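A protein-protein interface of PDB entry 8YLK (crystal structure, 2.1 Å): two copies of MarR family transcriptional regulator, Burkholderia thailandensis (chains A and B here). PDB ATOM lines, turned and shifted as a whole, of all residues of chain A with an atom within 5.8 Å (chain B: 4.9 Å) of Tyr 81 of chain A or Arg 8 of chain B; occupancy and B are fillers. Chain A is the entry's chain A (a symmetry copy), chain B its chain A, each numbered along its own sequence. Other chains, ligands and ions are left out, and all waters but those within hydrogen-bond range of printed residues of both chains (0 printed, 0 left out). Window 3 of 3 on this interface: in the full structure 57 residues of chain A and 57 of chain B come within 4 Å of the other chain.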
ATOM      1  N   ARG A  68      13.922  -5.826 -13.368  1.00  0.00           N
ATOM      2  CA  ARG A  68      15.053  -5.659 -14.271  1.00  0.00           C
ATOM      3  C   ARG A  68      16.108  -4.698 -13.734  1.00  0.00           C
ATOM      4  O   ARG A  68      17.121  -4.490 -14.410  1.00  0.00           O
ATOM      5  CB  ARG A  68      14.574  -5.198 -15.649  1.00  0.00           C
ATOM      6  CG  ARG A  68      13.882  -3.861 -15.663  1.00  0.00           C
ATOM      7  CD  ARG A  68      13.497  -3.477 -17.079  1.00  0.00           C
ATOM      8  NE  ARG A  68      12.297  -2.649 -17.108  1.00  0.00           N
ATOM      9  CZ  ARG A  68      12.266  -1.345 -16.838  1.00  0.00           C
ATOM     10  NH1 ARG A  68      13.377  -0.691 -16.514  1.00  0.00           N
ATOM     11  NH2 ARG A  68      11.112  -0.692 -16.893  1.00  0.00           N
ATOM     12  N   THR A  76      14.688   3.393  -4.985  1.00  0.00           N
ATOM     13  CA  THR A  76      13.989   4.545  -4.437  1.00  0.00           C
ATOM     14  C   THR A  76      12.773   4.848  -5.310  1.00  0.00           C
ATOM     15  O   THR A  76      12.751   4.504  -6.497  1.00  0.00           O
ATOM     16  CB  THR A  76      14.902   5.771  -4.378  1.00  0.00           C
ATOM     17  OG1 THR A  76      15.147   6.255  -5.703  1.00  0.00           O
ATOM     18  CG2 THR A  76      16.225   5.427  -3.718  1.00  0.00           C
ATOM     19  N   PRO A  77      11.737   5.483  -4.753  1.00  0.00           N
ATOM     20  CA  PRO A  77      10.579   5.833  -5.596  1.00  0.00           C
ATOM     21  C   PRO A  77      10.953   6.743  -6.753  1.00  0.00           C
ATOM     22  O   PRO A  77      10.273   6.743  -7.787  1.00  0.00           O
ATOM     23  CB  PRO A  77       9.618   6.516  -4.612  1.00  0.00           C
ATOM     24  CG  PRO A  77      10.066   6.059  -3.249  1.00  0.00           C
ATOM     25  CD  PRO A  77      11.551   5.900  -3.353  1.00  0.00           C
ATOM     26  N   THR A  78      12.038   7.501  -6.617  1.00  0.00           N
ATOM     27  CA  THR A  78      12.481   8.369  -7.700  1.00  0.00           C
ATOM     28  C   THR A  78      13.174   7.571  -8.795  1.00  0.00           C
ATOM     29  O   THR A  78      12.888   7.755  -9.983  1.00  0.00           O
ATOM     30  CB  THR A  78      13.407   9.451  -7.151  1.00  0.00           C
ATOM     31  OG1 THR A  78      12.692  10.230  -6.186  1.00  0.00           O
ATOM     32  CG2 THR A  78      13.891  10.358  -8.273  1.00  0.00           C
ATOM     33  N   ALA A  79      14.101   6.690  -8.412  1.00  0.00           N
ATOM     34  CA  ALA A  79      14.676   5.765  -9.382  1.00  0.00           C
ATOM     35  C   ALA A  79      13.586   4.935 -10.040  1.00  0.00           C
ATOM     36  O   ALA A  79      13.649   4.653 -11.243  1.00  0.00           O
ATOM     37  CB  ALA A  79      15.705   4.860  -8.703  1.00  0.00           C
ATOM     38  N   LEU A  80      12.569   4.553  -9.266  1.00  0.00           N
ATOM     39  CA  LEU A  80      11.452   3.789  -9.811  1.00  0.00           C
ATOM     40  C   LEU A  80      10.725   4.574 -10.896  1.00  0.00           C
ATOM     41  O   LEU A  80      10.351   4.015 -11.932  1.00  0.00           O
ATOM     42  CB  LEU A  80      10.503   3.398  -8.679  1.00  0.00           C
ATOM     43  CG  LEU A  80       9.313   2.477  -8.960  1.00  0.00           C
ATOM     44  CD1 LEU A  80       9.741   1.159  -9.597  1.00  0.00           C
ATOM     45  CD2 LEU A  80       8.549   2.225  -7.666  1.00  0.00           C
ATOM     46  N   TYR A  81      10.541   5.880 -10.695  1.00  0.00           N
ATOM     47  CA  TYR A  81       9.870   6.671 -11.720  1.00  0.00           C
ATOM     48  C   TYR A  81      10.752   6.860 -12.948  1.00  0.00           C
ATOM     49  O   TYR A  81      10.269   6.786 -14.084  1.00  0.00           O
ATOM     50  CB  TYR A  81       9.445   8.030 -11.172  1.00  0.00           C
ATOM     51  CG  TYR A  81       8.894   8.906 -12.270  1.00  0.00           C
ATOM     52  CD1 TYR A  81       7.567   8.799 -12.665  1.00  0.00           C
ATOM     53  CD2 TYR A  81       9.707   9.811 -12.943  1.00  0.00           C
ATOM     54  CE1 TYR A  81       7.060   9.585 -13.684  1.00  0.00           C
ATOM     55  CE2 TYR A  81       9.210  10.599 -13.964  1.00  0.00           C
ATOM     56  CZ  TYR A  81       7.886  10.485 -14.326  1.00  0.00           C
ATOM     57  OH  TYR A  81       7.389  11.268 -15.340  1.00  0.00           O
ATOM     58  N   ASP A  82      12.043   7.131 -12.744  1.00  0.00           N
ATOM     59  CA  ASP A  82      12.928   7.370 -13.879  1.00  0.00           C
ATOM     60  C   ASP A  82      13.137   6.111 -14.716  1.00  0.00           C
ATOM     61  O   ASP A  82      13.312   6.204 -15.936  1.00  0.00           O
ATOM     62  CB  ASP A  82      14.266   7.912 -13.387  1.00  0.00           C
ATOM     63  CG  ASP A  82      14.148   9.314 -12.844  1.00  0.00           C
ATOM     64  OD1 ASP A  82      13.283  10.064 -13.342  1.00  0.00           O
ATOM     65  OD2 ASP A  82      14.909   9.659 -11.919  1.00  0.00           O
ATOM     66  N   ALA A  83      13.115   4.939 -14.093  1.00  0.00           N
ATOM     67  CA  ALA A  83      13.338   3.693 -14.812  1.00  0.00           C
ATOM     68  C   ALA A  83      12.051   3.060 -15.319  1.00  0.00           C
ATOM     69  O   ALA A  83      12.112   2.034 -16.005  1.00  0.00           O
ATOM     70  CB  ALA A  83      14.090   2.696 -13.925  1.00  0.00           C
ATOM     71  N   ALA A  84      10.898   3.642 -15.002  1.00  0.00           N
ATOM     72  CA  ALA A  84       9.634   3.106 -15.486  1.00  0.00           C
ATOM     73  C   ALA A  84       9.594   3.129 -17.010  1.00  0.00           C
ATOM     74  O   ALA A  84      10.204   3.984 -17.656  1.00  0.00           O
ATOM     75  CB  ALA A  84       8.466   3.913 -14.920  1.00  0.00           C
ATOM     76  N   MET A  85       8.877   2.159 -17.587  1.00  0.00           N
ATOM     77  CA  MET A  85       8.680   2.155 -19.034  1.00  0.00           C
ATOM     78  C   MET A  85       7.785   3.308 -19.481  1.00  0.00           C
ATOM     79  O   MET A  85       8.020   3.910 -20.538  1.00  0.00           O
ATOM     80  CB  MET A  85       8.081   0.824 -19.480  1.00  0.00           C
ATOM     81  CG  MET A  85       7.630   0.812 -20.930  1.00  0.00           C
ATOM     82  SD  MET A  85       9.011   0.742 -22.087  1.00  0.00           S
ATOM     83  CE  MET A  85       9.546  -0.960 -21.874  1.00  0.00           C
ATOM     84  N   ILE A  86       6.754   3.622 -18.696  1.00  0.00           N
ATOM     85  CA  ILE A  86       5.755   4.631 -19.037  1.00  0.00           C
ATOM     86  C   ILE A  86       5.677   5.642 -17.897  1.00  0.00           C
ATOM     87  O   ILE A  86       5.557   5.259 -16.728  1.00  0.00           O
ATOM     88  CB  ILE A  86       4.378   3.989 -19.293  1.00  0.00           C
ATOM     89  CG1 ILE A  86       4.504   2.837 -20.294  1.00  0.00           C
ATOM     90  CG2 ILE A  86       3.404   5.015 -19.818  1.00  0.00           C
ATOM     91  CD1 ILE A  86       3.195   2.141 -20.595  1.00  0.00           C
ATOM     92  N   SER A  87       5.730   6.931 -18.234  1.00  0.00           N
ATOM     93  CA  SER A  87       5.721   7.957 -17.198  1.00  0.00           C
ATOM     94  C   SER A  87       4.305   8.281 -16.728  1.00  0.00           C
ATOM     95  O   SER A  87       3.915   9.451 -16.675  1.00  0.00           O
ATOM     96  CB  SER A  87       6.428   9.228 -17.690  1.00  0.00           C
ATOM     97  OG  SER A  87       5.747   9.816 -18.784  1.00  0.00           O
ATOM     98  N   SER A  88       3.527   7.258 -16.380  1.00  0.00           N
ATOM     99  CA  SER A  88       2.210   7.492 -15.807  1.00  0.00           C
ATOM    100  C   SER A  88       2.334   7.916 -14.342  1.00  0.00           C
ATOM    101  O   SER A  88       3.372   7.735 -13.697  1.00  0.00           O
ATOM    102  CB  SER A  88       1.333   6.244 -15.933  1.00  0.00           C
ATOM    103  OG  SER A  88       1.989   5.084 -15.445  1.00  0.00           O
ATOM    104  N   MET A  91       1.887   7.007  -8.687  1.00  0.00           N
ATOM    105  CA  MET A  91       2.877   6.011  -8.282  1.00  0.00           C
ATOM    106  C   MET A  91       2.732   5.637  -6.809  1.00  0.00           C
ATOM    107  O   MET A  91       2.938   4.475  -6.438  1.00  0.00           O
ATOM    108  CB  MET A  91       4.287   6.532  -8.572  1.00  0.00           C
ATOM    109  CG  MET A  91       5.415   5.582  -8.195  1.00  0.00           C
ATOM    110  SD  MET A  91       5.659   4.253  -9.387  1.00  0.00           S
ATOM    111  CE  MET A  91       6.370   5.126 -10.776  1.00  0.00           C
ATOM    112  N   MET B   6      19.830   6.838 -24.180  1.00  0.00           N
ATOM    113  CA  MET B   6      18.752   5.865 -24.349  1.00  0.00           C
ATOM    114  C   MET B   6      17.457   6.329 -23.693  1.00  0.00           C
ATOM    115  O   MET B   6      17.469   6.853 -22.579  1.00  0.00           O
ATOM    116  CB  MET B   6      19.150   4.506 -23.769  1.00  0.00           C
ATOM    117  CG  MET B   6      19.938   3.623 -24.715  1.00  0.00           C
ATOM    118  SD  MET B   6      19.972   1.913 -24.138  1.00  0.00           S
ATOM    119  CE  MET B   6      20.946   1.133 -25.423  1.00  0.00           C
ATOM    120  N   ASP B   7      16.340   6.120 -24.387  1.00  0.00           N
ATOM    121  CA  ASP B   7      15.038   6.443 -23.831  1.00  0.00           C
ATOM    122  C   ASP B   7      14.599   5.347 -22.860  1.00  0.00           C
ATOM    123  O   ASP B   7      15.321   4.378 -22.603  1.00  0.00           O
ATOM    124  CB  ASP B   7      14.011   6.644 -24.947  1.00  0.00           C
ATOM    125  CG  ASP B   7      13.647   5.345 -25.651  1.00  0.00           C
ATOM    126  OD1 ASP B   7      14.513   4.455 -25.755  1.00  0.00           O
ATOM    127  OD2 ASP B   7      12.493   5.217 -26.107  1.00  0.00           O
ATOM    128  N   ARG B   8      13.393   5.509 -22.310  1.00  0.00           N
ATOM    129  CA  ARG B   8      12.881   4.557 -21.328  1.00  0.00           C
ATOM    130  C   ARG B   8      12.799   3.150 -21.903  1.00  0.00           C
ATOM    131  O   ARG B   8      13.174   2.179 -21.237  1.00  0.00           O
ATOM    132  CB  ARG B   8      11.500   4.990 -20.834  1.00  0.00           C
ATOM    133  CG  ARG B   8      11.465   6.295 -20.067  1.00  0.00           C
ATOM    134  CD  ARG B   8      10.033   6.666 -19.727  1.00  0.00           C
ATOM    135  NE  ARG B   8       9.966   7.842 -18.866  1.00  0.00           N
ATOM    136  CZ  ARG B   8      10.026   7.790 -17.541  1.00  0.00           C
ATOM    137  NH1 ARG B   8      10.158   6.622 -16.925  1.00  0.00           N
ATOM    138  NH2 ARG B   8       9.963   8.907 -16.829  1.00  0.00           N
ATOM    139  N   ALA B   9      12.313   3.022 -23.140  1.00  0.00           N
ATOM    140  CA  ALA B   9      12.069   1.700 -23.703  1.00  0.00           C
ATOM    141  C   ALA B   9      13.374   0.976 -24.016  1.00  0.00           C
ATOM    142  O   ALA B   9      13.503  -0.225 -23.744  1.00  0.00           O
ATOM    143  CB  ALA B   9      11.195   1.819 -24.950  1.00  0.00           C
ATOM    144  N   ALA B  10      14.353   1.682 -24.588  1.00  0.00           N
ATOM    145  CA  ALA B  10      15.614   1.028 -24.921  1.00  0.00           C
ATOM    146  C   ALA B  10      16.393   0.669 -23.664  1.00  0.00           C
ATOM    147  O   ALA B  10      16.994  -0.409 -23.583  1.00  0.00           O
ATOM    148  CB  ALA B  10      16.444   1.920 -25.842  1.00  0.00           C
ATOM    149  N   HIS B  11      16.391   1.556 -22.669  1.00  0.00           N
ATOM    150  CA  HIS B  11      17.046   1.248 -21.405  1.00  0.00           C
ATOM    151  C   HIS B  11      16.397   0.044 -20.735  1.00  0.00           C
ATOM    152  O   HIS B  11      17.090  -0.810 -20.167  1.00  0.00           O
ATOM    153  CB  HIS B  11      17.002   2.467 -20.485  1.00  0.00           C
ATOM    154  CG  HIS B  11      17.641   2.243 -19.152  1.00  0.00           C
ATOM    155  ND1 HIS B  11      18.954   1.844 -19.014  1.00  0.00           N
ATOM    156  CD2 HIS B  11      17.149   2.362 -17.896  1.00  0.00           C
ATOM    157  CE1 HIS B  11      19.243   1.728 -17.730  1.00  0.00           C
ATOM    158  NE2 HIS B  11      18.166   2.038 -17.030  1.00  0.00           N
ATOM    159  N   ALA B  12      15.066  -0.044 -20.801  1.00  0.00           N
ATOM    160  CA  ALA B  12      14.365  -1.177 -20.205  1.00  0.00           C
ATOM    161  C   ALA B  12      14.733  -2.482 -20.903  1.00  0.00           C
ATOM    162  O   ALA B  12      15.044  -3.481 -20.247  1.00  0.00           O
ATOM    163  CB  ALA B  12      12.855  -0.940 -20.255  1.00  0.00           C
ATOM    164  N   GLU B  36       4.104   5.456 -24.529  1.00  0.00           N
ATOM    165  CA  GLU B  36       4.679   6.656 -23.928  1.00  0.00           C
ATOM    166  C   GLU B  36       4.436   7.883 -24.799  1.00  0.00           C
ATOM    167  O   GLU B  36       4.151   8.970 -24.282  1.00  0.00           O
ATOM    168  CB  GLU B  36       6.173   6.452 -23.676  1.00  0.00           C
ATOM    169  CG  GLU B  36       6.877   7.655 -23.052  1.00  0.00           C
ATOM    170  CD  GLU B  36       6.500   7.883 -21.596  1.00  0.00           C
ATOM    171  OE1 GLU B  36       5.597   7.189 -21.078  1.00  0.00           O
ATOM    172  OE2 GLU B  36       7.119   8.763 -20.967  1.00  0.00           O
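The backbone carbonyl oxygen of Tyr 81 of chain A sits at hydrogen-bond distance from the guanidinium group of Arg 8 of chain B, 2.8 Å away.
The guanidinium group (NH1) of Arg 8 of chain B lies within hydrogen-bond range of the backbone carbonyl oxygen (O) of Asp 82 of chain A, at 3.3 Å.
O of Ala 84 of chain A is in hydrogen-bond range of NH1 of Arg 8 of chain B (2.7 Å).
The side-chain carboxylate (OE2) of Glu 36 of chain B lies within hydrogen-bond range of the side-chain hydroxyl (OG) of Ser 87 of chain A (2.8 Å).
The guanidinium group of Arg 8 of chain B is in salt-bridge range of the side-chain carboxylate of Glu 36 of chain B, at 3.7 Å.
NH2 of Arg 68 of chain A lies within hydrogen-bond range of O of Ala 83 of chain A (3.0 Å).
Arg 68 of chain A touches Ala 12 of chain B.
Met 85 of chain A touches Arg 8 of chain B (O to CD, 3.5 Å).
Ala 9 of chain B touches Met 85 of chain A (CA to SD, 3.6 Å).
Met 85 of chain A touches Ala 12 of chain B.
Glu 36 of chain B touches Ile 86 of chain A (OE1 to CA, 3.3 Å).
NH2 of Arg 8 of chain B touches CB of Ser 87 of chain A, at 3.7 Å.
Of chain B, only Arg 8 comes within 4 Å of Tyr 81 of chain A.
Arg 8 of chain B touches five residues of chain A.
Of the printed residues of chain B, Arg 68 of chain A touches Ala 12 (3.5 Å).
Printed residues of chain A within 4 Å of Glu 36 of chain B: Ile 86 and Ser 87.
Of the printed residues of chain B, Ile 86 of chain A touches Glu 36.
Met 6 of chain B touches none of the printed residues of chain A.
His 11 of chain B touches none of the printed residues of chain A.
The nearest printed residue of chain B that does not touch Tyr 81 of chain A is Glu 36 of chain B (6.2 Å).
Of the 15 printed residues of chain A, 7 touch a printed residue of chain B.
Hydrophobic or aromatic side chains of chain A that line the printed part of chain B: Tyr 81, Ala 84, Met 85 and Ile 86.
Of the 8 printed residues of chain B, 4 touch a printed residue of chain A.
Along chain B the printed residues that touch a printed residue of chain A span positions 8 to 36.
Among the printed residues, 10 pairs touch across the chains.
Among the printed residues, no Asp or Glu carboxylate lies within 4 Å of a Lys or Arg side-chain nitrogen of the other chain.
No position is printed for both chains.
Of the 10 pairs that touch across the chains among the printed residues, none has its exchanged pair printed and touching as well.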
